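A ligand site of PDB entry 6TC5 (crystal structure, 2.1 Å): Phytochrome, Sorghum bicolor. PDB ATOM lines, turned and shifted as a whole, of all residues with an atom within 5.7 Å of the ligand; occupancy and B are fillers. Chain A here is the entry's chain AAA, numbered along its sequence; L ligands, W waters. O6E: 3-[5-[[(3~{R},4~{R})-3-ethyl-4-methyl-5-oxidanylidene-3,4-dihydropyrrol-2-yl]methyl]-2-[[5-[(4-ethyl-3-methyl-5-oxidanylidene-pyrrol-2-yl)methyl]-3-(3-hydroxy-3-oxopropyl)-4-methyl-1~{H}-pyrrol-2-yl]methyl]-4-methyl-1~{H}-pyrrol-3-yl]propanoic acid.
SG of Cys 262 is bonded to CAC of the ligand. The backbone NH of His 260 is in hydrogen-bond range of an oxygen (OBG) of the ligand (2.9 Å). A ring nitrogen (NE2) of His 309 is in hydrogen-bond range of an oxygen (OAK) of the ligand. A nitrogen (NAN) of the ligand is in hydrogen-bond range of the backbone carbonyl oxygen (O) of Asp 212 (3.0 Å). The guanidinium group of Arg 257 is in salt-bridge range of an oxygen (OBG) of the ligand (3.0 Å). OAZ of the ligand lies within salt-bridge range of NH1 of Arg 227 (3.0 Å). A ring nitrogen (ND1) of His 263 sits at hydrogen-bond distance from a nitrogen (NAE) of the ligand (3.3 Å).
Water W3 lies within hydrogen-bond range of an oxygen (OBF) of the ligand (2.6 Å), the side-chain hydroxyl of Ser 275 (2.7 Å) and the backbone carbonyl oxygen of Arg 227 (2.7 Å). Water W4 bridges the side-chain hydroxyl of Ser 217 and an oxygen (OBA) of the ligand. Water W1 lies within hydrogen-bond range of the side-chain hydroxyl (OG) of Ser 275, an oxygen (OBF) of the ligand and a ring nitrogen (NE2) of His 263. Water W2 lies within hydrogen-bond range of a nitrogen (NBP) of the ligand (2.7 Å), a ring nitrogen (ND1) of His 263 (2.8 Å) and the backbone carbonyl oxygen (O) of Asp 212 (3.0 Å). Water W5 bridges NAJ of the ligand (2.9 Å) and NE2 of His 309 (3.2 Å).
A ring nitrogen (ND1) of His 260 lies within hydrogen-bond range of the backbone NH (N) of Cys 262 (3.0 Å). OD2 of Asp 212 is in hydrogen-bond range of OH of Tyr 266, at 2.8 Å. O of Arg 257 lies within hydrogen-bond range of NH2 of Arg 227 (3.0 Å). O of Val 277 sits at hydrogen-bond distance from N of Arg 227 (2.9 Å). SD of Met 267 lies close to NE2 of His 263, at 3.5 Å. The backbone NH of Tyr 181 lies within hydrogen-bond range of the backbone carbonyl oxygen of Leu 305. O of Val 307 sits at hydrogen-bond distance from N of Met 179 (2.8 Å). N of Ser 275 sits at hydrogen-bond distance from O of Ile 229, at 2.9 Å.
The side-chain sulfur of Met 270 lies close to an oxygen (OAK) of the ligand. Tyr 5 touches the ligand (OH to CAH, 3.2 Å). OH of Tyr 181 touches CAS of the ligand (3.4 Å). CZ of Tyr 208 touches CAG of the ligand (3.6 Å). O of Thr 211 touches CAT of the ligand, at 3.7 Å. Ile 213 touches the ligand (CG1 to CBL, 3.4 Å). CD of Pro 214 touches NAN of the ligand, 3.4 Å away. OG of Ser 217 touches CAO of the ligand (3.8 Å). Phe 221 touches the ligand (CZ to OAZ, 3.4 Å). CD1 of Ile 229 touches OBF of the ligand, at 3.8 Å. Pro 259 touches the ligand (CA to OBG, 3.4 Å). OH of Tyr 266 touches CAS of the ligand, 3.1 Å away. Ser 275 touches the ligand (OG to OBF, 3.9 Å). Val 277 touches the ligand. Val 307 touches the ligand. Within 4 Å of the ligand: Tyr 5, Tyr 181, Tyr 208, Thr 211, Asp 212, Ile 213, Pro 214, Ser 217, Phe 221, Arg 227, Ile 229, Arg 257, Pro 259, His 260, Cys 262, His 263, Tyr 266, Met 270, Ser 275, Val 277, Val 307 and His 309.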
ATOM      1  N   TYR A   5     -28.660 -27.474   1.325  1.00  0.00           N
ATOM      2  CA  TYR A   5     -28.409 -26.280   2.221  1.00  0.00           C
ATOM      3  C   TYR A   5     -29.714 -25.690   2.798  1.00  0.00           C
ATOM      4  O   TYR A   5     -29.771 -25.540   4.018  1.00  0.00           O
ATOM      5  CB  TYR A   5     -27.606 -25.140   1.593  1.00  0.00           C
ATOM      6  CG  TYR A   5     -26.129 -25.390   1.393  1.00  0.00           C
ATOM      7  CD1 TYR A   5     -25.327 -25.936   2.381  1.00  0.00           C
ATOM      8  CD2 TYR A   5     -25.534 -25.084   0.186  1.00  0.00           C
ATOM      9  CE1 TYR A   5     -23.966 -26.167   2.169  1.00  0.00           C
ATOM     10  CE2 TYR A   5     -24.193 -25.315  -0.046  1.00  0.00           C
ATOM     11  CZ  TYR A   5     -23.398 -25.838   0.950  1.00  0.00           C
ATOM     12  OH  TYR A   5     -22.067 -26.038   0.667  1.00  0.00           O
ATOM     13  N   ILE A   9     -30.581 -25.079   6.812  1.00  0.00           N
ATOM     14  CA  ILE A   9     -30.525 -23.720   7.402  1.00  0.00           C
ATOM     15  C   ILE A   9     -31.889 -23.390   8.028  1.00  0.00           C
ATOM     16  O   ILE A   9     -31.920 -22.792   9.123  1.00  0.00           O
ATOM     17  CB  ILE A   9     -30.126 -22.695   6.326  1.00  0.00           C
ATOM     18  CG1 ILE A   9     -28.709 -22.946   5.798  1.00  0.00           C
ATOM     19  CG2 ILE A   9     -30.289 -21.284   6.860  1.00  0.00           C
ATOM     20  CD1 ILE A   9     -28.393 -22.203   4.509  1.00  0.00           C
ATOM     21  N   MET A 179     -16.665  -4.575   7.409  1.00  0.00           N
ATOM     22  CA  MET A 179     -16.438  -4.537   5.950  1.00  0.00           C
ATOM     23  C   MET A 179     -17.756  -4.350   5.193  1.00  0.00           C
ATOM     24  O   MET A 179     -18.831  -4.815   5.662  1.00  0.00           O
ATOM     25  CB  MET A 179     -15.785  -5.839   5.498  1.00  0.00           C
ATOM     26  CG  MET A 179     -14.438  -6.140   6.152  1.00  0.00           C
ATOM     27  SD  MET A 179     -13.921  -7.849   5.736  1.00  0.00           S
ATOM     28  CE  MET A 179     -15.010  -8.820   6.759  1.00  0.00           C
ATOM     29  N   TYR A 181     -19.040  -5.893   1.810  1.00  0.00           N
ATOM     30  CA  TYR A 181     -18.826  -6.988   0.835  1.00  0.00           C
ATOM     31  C   TYR A 181     -19.800  -6.787  -0.334  1.00  0.00           C
ATOM     32  O   TYR A 181     -20.994  -6.943  -0.107  1.00  0.00           O
ATOM     33  CB  TYR A 181     -19.045  -8.310   1.557  1.00  0.00           C
ATOM     34  CG  TYR A 181     -18.657  -9.525   0.799  1.00  0.00           C
ATOM     35  CD1 TYR A 181     -17.357  -9.986   0.834  1.00  0.00           C
ATOM     36  CD2 TYR A 181     -19.584 -10.280   0.104  1.00  0.00           C
ATOM     37  CE1 TYR A 181     -16.982 -11.138   0.172  1.00  0.00           C
ATOM     38  CE2 TYR A 181     -19.230 -11.445  -0.536  1.00  0.00           C
ATOM     39  CZ  TYR A 181     -17.920 -11.882  -0.511  1.00  0.00           C
ATOM     40  OH  TYR A 181     -17.530 -13.028  -1.147  1.00  0.00           O
ATOM     41  N   VAL A 191     -14.338  -7.235  -0.949  1.00  0.00           N
ATOM     42  CA  VAL A 191     -14.341  -6.274   0.191  1.00  0.00           C
ATOM     43  C   VAL A 191     -14.007  -4.885  -0.382  1.00  0.00           C
ATOM     44  O   VAL A 191     -12.847  -4.661  -0.809  1.00  0.00           O
ATOM     45  CB  VAL A 191     -13.348  -6.729   1.268  1.00  0.00           C
ATOM     46  CG1 VAL A 191     -13.286  -5.784   2.452  1.00  0.00           C
ATOM     47  CG2 VAL A 191     -13.626  -8.161   1.720  1.00  0.00           C
ATOM     48  N   TYR A 203      -8.465  -7.031   4.924  1.00  0.00           N
ATOM     49  CA  TYR A 203      -9.087  -7.802   3.806  1.00  0.00           C
ATOM     50  C   TYR A 203      -9.507  -6.862   2.687  1.00  0.00           C
ATOM     51  O   TYR A 203      -9.988  -7.354   1.679  1.00  0.00           O
ATOM     52  CB  TYR A 203     -10.304  -8.586   4.278  1.00  0.00           C
ATOM     53  CG  TYR A 203     -10.013  -9.592   5.347  1.00  0.00           C
ATOM     54  CD1 TYR A 203      -8.717 -10.016   5.653  1.00  0.00           C
ATOM     55  CD2 TYR A 203     -11.054 -10.167   6.035  1.00  0.00           C
ATOM     56  CE1 TYR A 203      -8.485 -10.963   6.631  1.00  0.00           C
ATOM     57  CE2 TYR A 203     -10.845 -11.092   7.038  1.00  0.00           C
ATOM     58  CZ  TYR A 203      -9.560 -11.499   7.336  1.00  0.00           C
ATOM     59  OH  TYR A 203      -9.439 -12.439   8.317  1.00  0.00           O
ATOM     60  N   TYR A 208     -13.540 -13.061  -3.227  1.00  0.00           N
ATOM     61  CA  TYR A 208     -13.899 -14.395  -2.708  1.00  0.00           C
ATOM     62  C   TYR A 208     -14.887 -15.039  -3.666  1.00  0.00           C
ATOM     63  O   TYR A 208     -15.739 -14.333  -4.241  1.00  0.00           O
ATOM     64  CB  TYR A 208     -14.424 -14.259  -1.274  1.00  0.00           C
ATOM     65  CG  TYR A 208     -13.452 -13.634  -0.299  1.00  0.00           C
ATOM     66  CD1 TYR A 208     -13.354 -12.264  -0.194  1.00  0.00           C
ATOM     67  CD2 TYR A 208     -12.685 -14.399   0.550  1.00  0.00           C
ATOM     68  CE1 TYR A 208     -12.490 -11.674   0.708  1.00  0.00           C
ATOM     69  CE2 TYR A 208     -11.813 -13.828   1.475  1.00  0.00           C
ATOM     70  CZ  TYR A 208     -11.725 -12.451   1.549  1.00  0.00           C
ATOM     71  OH  TYR A 208     -10.871 -11.819   2.422  1.00  0.00           O
ATOM     72  N   PRO A 209     -14.781 -16.366  -3.872  1.00  0.00           N
ATOM     73  CA  PRO A 209     -15.666 -17.096  -4.775  1.00  0.00           C
ATOM     74  C   PRO A 209     -17.148 -17.007  -4.397  1.00  0.00           C
ATOM     75  O   PRO A 209     -17.478 -17.011  -3.208  1.00  0.00           O
ATOM     76  CB  PRO A 209     -15.267 -18.573  -4.643  1.00  0.00           C
ATOM     77  CG  PRO A 209     -13.948 -18.599  -3.875  1.00  0.00           C
ATOM     78  CD  PRO A 209     -13.786 -17.233  -3.223  1.00  0.00           C
ATOM     79  N   THR A 211     -19.328 -19.233  -4.352  1.00  0.00           N
ATOM     80  CA  THR A 211     -19.729 -20.459  -3.625  1.00  0.00           C
ATOM     81  C   THR A 211     -19.389 -20.363  -2.145  1.00  0.00           C
ATOM     82  O   THR A 211     -19.859 -21.230  -1.382  1.00  0.00           O
ATOM     83  CB  THR A 211     -19.099 -21.700  -4.246  1.00  0.00           C
ATOM     84  OG1 THR A 211     -17.717 -21.416  -4.434  1.00  0.00           O
ATOM     85  CG2 THR A 211     -19.754 -22.091  -5.552  1.00  0.00           C
ATOM     86  N   ASP A 212     -18.662 -19.343  -1.699  1.00  0.00           N
ATOM     87  CA  ASP A 212     -18.407 -19.163  -0.242  1.00  0.00           C
ATOM     88  C   ASP A 212     -19.730 -18.813   0.454  1.00  0.00           C
ATOM     89  O   ASP A 212     -19.834 -19.041   1.689  1.00  0.00           O
ATOM     90  CB  ASP A 212     -17.371 -18.070   0.064  1.00  0.00           C
ATOM     91  CG  ASP A 212     -15.926 -18.454  -0.247  1.00  0.00           C
ATOM     92  OD1 ASP A 212     -15.722 -19.507  -0.944  1.00  0.00           O
ATOM     93  OD2 ASP A 212     -15.034 -17.697   0.156  1.00  0.00           O
ATOM     94  N   ILE A 213     -20.645 -18.191  -0.302  1.00  0.00           N
ATOM     95  CA  ILE A 213     -22.007 -17.797   0.190  1.00  0.00           C
ATOM     96  C   ILE A 213     -23.021 -18.455  -0.731  1.00  0.00           C
ATOM     97  O   ILE A 213     -23.407 -17.902  -1.736  1.00  0.00           O
ATOM     98  CB  ILE A 213     -22.213 -16.265   0.276  1.00  0.00           C
ATOM     99  CG1 ILE A 213     -21.072 -15.598   1.054  1.00  0.00           C
ATOM    100  CG2 ILE A 213     -23.591 -15.965   0.897  1.00  0.00           C
ATOM    101  CD1 ILE A 213     -21.167 -14.091   1.136  1.00  0.00           C
ATOM    102  N   PRO A 214     -23.518 -19.658  -0.404  1.00  0.00           N
ATOM    103  CA  PRO A 214     -24.486 -20.329  -1.271  1.00  0.00           C
ATOM    104  C   PRO A 214     -25.717 -19.457  -1.569  1.00  0.00           C
ATOM    105  O   PRO A 214     -26.050 -18.571  -0.790  1.00  0.00           O
ATOM    106  CB  PRO A 214     -24.931 -21.544  -0.466  1.00  0.00           C
ATOM    107  CG  PRO A 214     -23.816 -21.766   0.546  1.00  0.00           C
ATOM    108  CD  PRO A 214     -23.251 -20.397   0.836  1.00  0.00           C
ATOM    109  N   SER A 217     -28.217 -19.010   1.297  1.00  0.00           N
ATOM    110  CA  SER A 217     -27.802 -18.017   2.307  1.00  0.00           C
ATOM    111  C   SER A 217     -28.145 -16.618   1.747  1.00  0.00           C
ATOM    112  O   SER A 217     -28.790 -15.805   2.454  1.00  0.00           O
ATOM    113  CB  SER A 217     -26.342 -18.167   2.700  1.00  0.00           C
ATOM    114  OG  SER A 217     -25.920 -17.058   3.508  1.00  0.00           O
ATOM    115  N   PHE A 221     -31.216 -13.782   3.349  1.00  0.00           N
ATOM    116  CA  PHE A 221     -30.883 -12.409   3.803  1.00  0.00           C
ATOM    117  C   PHE A 221     -31.920 -11.371   3.373  1.00  0.00           C
ATOM    118  O   PHE A 221     -31.936 -10.270   3.965  1.00  0.00           O
ATOM    119  CB  PHE A 221     -29.480 -12.045   3.326  1.00  0.00           C
ATOM    120  CG  PHE A 221     -28.425 -12.391   4.338  1.00  0.00           C
ATOM    121  CD1 PHE A 221     -28.403 -11.763   5.572  1.00  0.00           C
ATOM    122  CD2 PHE A 221     -27.439 -13.334   4.062  1.00  0.00           C
ATOM    123  CE1 PHE A 221     -27.447 -12.092   6.524  1.00  0.00           C
ATOM    124  CE2 PHE A 221     -26.480 -13.663   5.000  1.00  0.00           C
ATOM    125  CZ  PHE A 221     -26.500 -13.065   6.237  1.00  0.00           C
ATOM    126  N   ARG A 227     -27.933 -11.176  11.094  1.00  0.00           N
ATOM    127  CA  ARG A 227     -27.557 -12.491  11.631  1.00  0.00           C
ATOM    128  C   ARG A 227     -26.310 -12.311  12.497  1.00  0.00           C
ATOM    129  O   ARG A 227     -25.272 -11.879  11.974  1.00  0.00           O
ATOM    130  CB  ARG A 227     -27.378 -13.419  10.419  1.00  0.00           C
ATOM    131  CG  ARG A 227     -27.652 -14.875  10.703  1.00  0.00           C
ATOM    132  CD  ARG A 227     -26.614 -15.399  11.669  1.00  0.00           C
ATOM    133  NE  ARG A 227     -26.867 -16.788  12.014  1.00  0.00           N
ATOM    134  CZ  ARG A 227     -26.524 -17.815  11.264  1.00  0.00           C
ATOM    135  NH1 ARG A 227     -25.902 -17.626  10.100  1.00  0.00           N
ATOM    136  NH2 ARG A 227     -26.800 -19.015  11.717  1.00  0.00           N
ATOM    137  N   ILE A 229     -23.553 -14.409  15.036  1.00  0.00           N
ATOM    138  CA  ILE A 229     -22.946 -15.668  15.567  1.00  0.00           C
ATOM    139  C   ILE A 229     -21.969 -15.270  16.688  1.00  0.00           C
ATOM    140  O   ILE A 229     -21.059 -14.442  16.436  1.00  0.00           O
ATOM    141  CB  ILE A 229     -22.292 -16.494  14.461  1.00  0.00           C
ATOM    142  CG1 ILE A 229     -23.320 -16.879  13.394  1.00  0.00           C
ATOM    143  CG2 ILE A 229     -21.629 -17.719  15.066  1.00  0.00           C
ATOM    144  CD1 ILE A 229     -22.714 -17.359  12.066  1.00  0.00           C
ATOM    145  N   ARG A 257     -30.319 -18.960  15.785  1.00  0.00           N
ATOM    146  CA  ARG A 257     -30.143 -20.137  14.891  1.00  0.00           C
ATOM    147  C   ARG A 257     -28.634 -20.494  14.780  1.00  0.00           C
ATOM    148  O   ARG A 257     -27.834 -19.617  14.512  1.00  0.00           O
ATOM    149  CB  ARG A 257     -30.766 -19.783  13.540  1.00  0.00           C
ATOM    150  CG  ARG A 257     -30.509 -20.806  12.449  1.00  0.00           C
ATOM    151  CD  ARG A 257     -31.233 -20.456  11.183  1.00  0.00           C
ATOM    152  NE  ARG A 257     -30.744 -19.349  10.381  1.00  0.00           N
ATOM    153  CZ  ARG A 257     -29.610 -19.344   9.693  1.00  0.00           C
ATOM    154  NH1 ARG A 257     -29.301 -18.294   8.946  1.00  0.00           N
ATOM    155  NH2 ARG A 257     -28.783 -20.387   9.737  1.00  0.00           N
ATOM    156  N   ALA A 258     -28.245 -21.756  14.995  1.00  0.00           N
ATOM    157  CA  ALA A 258     -26.841 -22.206  14.911  1.00  0.00           C
ATOM    158  C   ALA A 258     -26.383 -22.137  13.466  1.00  0.00           C
ATOM    159  O   ALA A 258     -27.143 -22.462  12.569  1.00  0.00           O
ATOM    160  CB  ALA A 258     -26.672 -23.616  15.428  1.00  0.00           C
ATOM    161  N   PRO A 259     -25.143 -21.714  13.172  1.00  0.00           N
ATOM    162  CA  PRO A 259     -24.673 -21.699  11.785  1.00  0.00           C
ATOM    163  C   PRO A 259     -24.439 -23.105  11.218  1.00  0.00           C
ATOM    164  O   PRO A 259     -23.999 -23.949  11.969  1.00  0.00           O
ATOM    165  CB  PRO A 259     -23.343 -20.966  11.913  1.00  0.00           C
ATOM    166  CG  PRO A 259     -22.876 -21.317  13.307  1.00  0.00           C
ATOM    167  CD  PRO A 259     -24.131 -21.290  14.143  1.00  0.00           C
ATOM    168  N   HIS A 260     -24.723 -23.324   9.926  1.00  0.00           N
ATOM    169  CA  HIS A 260     -24.320 -24.576   9.213  1.00  0.00           C
ATOM    170  C   HIS A 260     -22.855 -24.865   9.518  1.00  0.00           C
ATOM    171  O   HIS A 260     -22.001 -23.897   9.531  1.00  0.00           O
ATOM    172  CB  HIS A 260     -24.574 -24.442   7.717  1.00  0.00           C
ATOM    173  CG  HIS A 260     -24.427 -25.713   6.956  1.00  0.00           C
ATOM    174  ND1 HIS A 260     -23.205 -26.383   6.835  1.00  0.00           N
ATOM    175  CD2 HIS A 260     -25.325 -26.430   6.241  1.00  0.00           C
ATOM    176  CE1 HIS A 260     -23.375 -27.455   6.090  1.00  0.00           C
ATOM    177  NE2 HIS A 260     -24.659 -27.501   5.705  1.00  0.00           N
ATOM    178  N   CYS A 262     -20.411 -26.138   7.932  1.00  0.00           N
ATOM    179  CA  CYS A 262     -19.413 -25.710   6.939  1.00  0.00           C
ATOM    180  C   CYS A 262     -18.988 -24.268   7.245  1.00  0.00           C
ATOM    181  O   CYS A 262     -17.768 -23.990   7.360  1.00  0.00           O
ATOM    182  CB  CYS A 262     -19.976 -25.797   5.530  1.00  0.00           C
ATOM    183  SG  CYS A 262     -18.776 -25.188   4.336  1.00  0.00           S
ATOM    184  N   HIS A 263     -19.959 -23.387   7.411  1.00  0.00           N
ATOM    185  CA  HIS A 263     -19.704 -21.957   7.711  1.00  0.00           C
ATOM    186  C   HIS A 263     -19.030 -21.801   9.086  1.00  0.00           C
ATOM    187  O   HIS A 263     -18.139 -20.957   9.173  1.00  0.00           O
ATOM    188  CB  HIS A 263     -20.956 -21.107   7.588  1.00  0.00           C
ATOM    189  CG  HIS A 263     -20.605 -19.672   7.766  1.00  0.00           C
ATOM    190  ND1 HIS A 263     -19.798 -19.015   6.852  1.00  0.00           N
ATOM    191  CD2 HIS A 263     -20.862 -18.818   8.773  1.00  0.00           C
ATOM    192  CE1 HIS A 263     -19.619 -17.786   7.281  1.00  0.00           C
ATOM    193  NE2 HIS A 263     -20.265 -17.646   8.454  1.00  0.00           N
ATOM    194  N   TYR A 266     -15.551 -22.443   8.337  1.00  0.00           N
ATOM    195  CA  TYR A 266     -15.054 -21.328   7.487  1.00  0.00           C
ATOM    196  C   TYR A 266     -14.657 -20.150   8.373  1.00  0.00           C
ATOM    197  O   TYR A 266     -13.628 -19.448   8.099  1.00  0.00           O
ATOM    198  CB  TYR A 266     -16.144 -20.888   6.524  1.00  0.00           C
ATOM    199  CG  TYR A 266     -15.738 -19.800   5.563  1.00  0.00           C
ATOM    200  CD1 TYR A 266     -15.217 -20.113   4.305  1.00  0.00           C
ATOM    201  CD2 TYR A 266     -15.915 -18.459   5.885  1.00  0.00           C
ATOM    202  CE1 TYR A 266     -14.878 -19.123   3.395  1.00  0.00           C
ATOM    203  CE2 TYR A 266     -15.580 -17.452   4.989  1.00  0.00           C
ATOM    204  CZ  TYR A 266     -15.056 -17.789   3.737  1.00  0.00           C
ATOM    205  OH  TYR A 266     -14.755 -16.825   2.845  1.00  0.00           O
ATOM    206  N   MET A 267     -15.482 -19.888   9.387  1.00  0.00           N
ATOM    207  CA  MET A 267     -15.271 -18.785  10.355  1.00  0.00           C
ATOM    208  C   MET A 267     -13.973 -19.062  11.152  1.00  0.00           C
ATOM    209  O   MET A 267     -13.134 -18.162  11.223  1.00  0.00           O
ATOM    210  CB  MET A 267     -16.468 -18.675  11.305  1.00  0.00           C
ATOM    211  CG  MET A 267     -17.679 -18.060  10.646  1.00  0.00           C
ATOM    212  SD  MET A 267     -19.112 -17.859  11.764  1.00  0.00           S
ATOM    213  CE  MET A 267     -18.511 -16.622  12.907  1.00  0.00           C
ATOM    214  N   MET A 270     -10.973 -18.601   9.092  1.00  0.00           N
ATOM    215  CA  MET A 270     -10.727 -17.182   8.733  1.00  0.00           C
ATOM    216  C   MET A 270     -10.245 -16.420   9.999  1.00  0.00           C
ATOM    217  O   MET A 270      -9.792 -15.303   9.831  1.00  0.00           O
ATOM    218  CB  MET A 270     -12.009 -16.574   8.158  1.00  0.00           C
ATOM    219  CG  MET A 270     -11.865 -15.190   7.619  1.00  0.00           C
ATOM    220  SD  MET A 270     -13.299 -14.683   6.629  1.00  0.00           S
ATOM    221  CE  MET A 270     -12.922 -15.449   5.067  1.00  0.00           C
ATOM    222  N   SER A 275     -19.398 -13.063  14.550  1.00  0.00           N
ATOM    223  CA  SER A 275     -19.752 -12.257  13.381  1.00  0.00           C
ATOM    224  C   SER A 275     -21.100 -11.584  13.573  1.00  0.00           C
ATOM    225  O   SER A 275     -21.927 -12.068  14.356  1.00  0.00           O
ATOM    226  CB  SER A 275     -19.691 -13.093  12.109  1.00  0.00           C
ATOM    227  OG  SER A 275     -20.660 -14.125  12.122  1.00  0.00           O
ATOM    228  N   VAL A 277     -23.585 -10.036  10.496  1.00  0.00           N
ATOM    229  CA  VAL A 277     -23.719  -9.869   9.038  1.00  0.00           C
ATOM    230  C   VAL A 277     -25.109  -9.311   8.740  1.00  0.00           C
ATOM    231  O   VAL A 277     -26.108  -9.814   9.312  1.00  0.00           O
ATOM    232  CB  VAL A 277     -23.455 -11.197   8.338  1.00  0.00           C
ATOM    233  CG1 VAL A 277     -23.622 -11.042   6.843  1.00  0.00           C
ATOM    234  CG2 VAL A 277     -22.079 -11.742   8.692  1.00  0.00           C
ATOM    235  N   LEU A 305     -23.320  -7.087   1.649  1.00  0.00           N
ATOM    236  CA  LEU A 305     -23.427  -7.402   3.082  1.00  0.00           C
ATOM    237  C   LEU A 305     -22.533  -6.419   3.813  1.00  0.00           C
ATOM    238  O   LEU A 305     -21.426  -6.094   3.299  1.00  0.00           O
ATOM    239  CB  LEU A 305     -22.957  -8.841   3.313  1.00  0.00           C
ATOM    240  CG  LEU A 305     -23.780  -9.964   2.670  1.00  0.00           C
ATOM    241  CD1 LEU A 305     -23.066 -11.304   2.871  1.00  0.00           C
ATOM    242  CD2 LEU A 305     -25.194 -10.050   3.242  1.00  0.00           C
ATOM    243  N   VAL A 307     -20.294  -6.977   6.779  1.00  0.00           N
ATOM    244  CA  VAL A 307     -19.744  -8.139   7.514  1.00  0.00           C
ATOM    245  C   VAL A 307     -18.895  -7.628   8.677  1.00  0.00           C
ATOM    246  O   VAL A 307     -17.936  -6.900   8.394  1.00  0.00           O
ATOM    247  CB  VAL A 307     -18.913  -9.018   6.571  1.00  0.00           C
ATOM    248  CG1 VAL A 307     -18.310 -10.163   7.341  1.00  0.00           C
ATOM    249  CG2 VAL A 307     -19.722  -9.520   5.374  1.00  0.00           C
ATOM    250  N   HIS A 309     -16.573  -8.899  12.062  1.00  0.00           N
ATOM    251  CA  HIS A 309     -15.840 -10.025  12.697  1.00  0.00           C
ATOM    252  C   HIS A 309     -15.253  -9.593  14.032  1.00  0.00           C
ATOM    253  O   HIS A 309     -14.906  -8.405  14.171  1.00  0.00           O
ATOM    254  CB  HIS A 309     -14.714 -10.543  11.827  1.00  0.00           C
ATOM    255  CG  HIS A 309     -15.144 -11.145  10.540  1.00  0.00           C
ATOM    256  ND1 HIS A 309     -14.264 -11.358   9.521  1.00  0.00           N
ATOM    257  CD2 HIS A 309     -16.346 -11.626  10.146  1.00  0.00           C
ATOM    258  CE1 HIS A 309     -14.900 -11.921   8.522  1.00  0.00           C
ATOM    259  NE2 HIS A 309     -16.179 -12.117   8.879  1.00  0.00           N
HETATM  260  CAH O6E L   1     -19.346 -26.651   2.172  1.00  0.00           C
HETATM  261  CAC O6E L   1     -19.558 -25.292   2.880  1.00  0.00           C
HETATM  262  CBJ O6E L   1     -19.537 -24.097   1.884  1.00  0.00           C
HETATM  263  CBD O6E L   1     -18.067 -23.755   1.553  1.00  0.00           C
HETATM  264  CAT O6E L   1     -17.714 -23.860   0.043  1.00  0.00           C
HETATM  265  CAX O6E L   1     -17.967 -22.298   2.087  1.00  0.00           C
HETATM  266  OBQ O6E L   1     -16.922 -21.651   2.082  1.00  0.00           O
HETATM  267  NBP O6E L   1     -19.107 -21.863   2.643  1.00  0.00           N
HETATM  268  CBN O6E L   1     -20.064 -22.791   2.563  1.00  0.00           C
HETATM  269  CAQ O6E L   1     -21.313 -22.692   3.056  1.00  0.00           C
HETATM  270  CAY O6E L   1     -21.913 -21.634   3.665  1.00  0.00           C
HETATM  271  NAN O6E L   1     -21.563 -20.327   3.740  1.00  0.00           N
HETATM  272  CBE O6E L   1     -23.130 -21.759   4.246  1.00  0.00           C
HETATM  273  CAU O6E L   1     -23.926 -23.123   4.330  1.00  0.00           C
HETATM  274  CBK O6E L   1     -23.507 -20.568   4.714  1.00  0.00           C
HETATM  275  CAD O6E L   1     -24.803 -20.317   5.453  1.00  0.00           C
HETATM  276  CAI O6E L   1     -24.521 -20.516   6.980  1.00  0.00           C
HETATM  277  CAM O6E L   1     -25.812 -20.265   7.837  1.00  0.00           C
HETATM  278  OBG O6E L   1     -26.051 -21.080   8.695  1.00  0.00           O
HETATM  279  OBA O6E L   1     -26.585 -19.312   7.581  1.00  0.00           O
HETATM  280  CBO O6E L   1     -22.530 -19.659   4.425  1.00  0.00           C
HETATM  281  CAO O6E L   1     -22.621 -18.329   4.788  1.00  0.00           C
HETATM  282  CAV O6E L   1     -21.712 -17.328   4.664  1.00  0.00           C
HETATM  283  NAE O6E L   1     -20.497 -17.323   4.053  1.00  0.00           N
HETATM  284  CBB O6E L   1     -21.912 -16.042   5.122  1.00  0.00           C
HETATM  285  CAA O6E L   1     -23.150 -15.493   5.844  1.00  0.00           C
HETATM  286  CAF O6E L   1     -22.972 -16.101   7.261  1.00  0.00           C
HETATM  287  CAL O6E L   1     -23.792 -15.360   8.314  1.00  0.00           C
HETATM  288  OBF O6E L   1     -23.241 -14.846   9.289  1.00  0.00           O
HETATM  289  OAZ O6E L   1     -24.993 -15.446   8.201  1.00  0.00           O
HETATM  290  CBH O6E L   1     -20.821 -15.285   4.844  1.00  0.00           C
HETATM  291  CAR O6E L   1     -20.692 -13.776   5.184  1.00  0.00           C
HETATM  292  CBL O6E L   1     -19.912 -16.080   4.210  1.00  0.00           C
HETATM  293  CAP O6E L   1     -18.680 -15.771   3.666  1.00  0.00           C
HETATM  294  CAW O6E L   1     -17.810 -14.781   4.013  1.00  0.00           C
HETATM  295  CBC O6E L   1     -16.858 -14.272   3.182  1.00  0.00           C
HETATM  296  CAS O6E L   1     -16.640 -14.668   1.708  1.00  0.00           C
HETATM  297  NAJ O6E L   1     -17.649 -14.168   5.214  1.00  0.00           N
HETATM  298  CBM O6E L   1     -16.626 -13.277   5.081  1.00  0.00           C
HETATM  299  OAK O6E L   1     -16.228 -12.564   6.003  1.00  0.00           O
HETATM  300  CBI O6E L   1     -16.105 -13.343   3.825  1.00  0.00           C
HETATM  301  CAB O6E L   1     -15.082 -12.654   3.249  1.00  0.00           C
HETATM  302  CAG O6E L   1     -14.238 -11.579   3.952  1.00  0.00           C
HETATM  303  O   HOH W   1     -20.555 -15.012   9.583  1.00  0.00           O
HETATM  304  O   HOH W   2     -18.765 -19.796   4.375  1.00  0.00           O
HETATM  305  O   HOH W   3     -23.234 -13.593  11.580  1.00  0.00           O
HETATM  306  O   HOH W   4     -26.320 -17.063   6.144  1.00  0.00           O
HETATM  307  O   HOH W   5     -18.293 -14.379   8.033  1.00  0.00           O
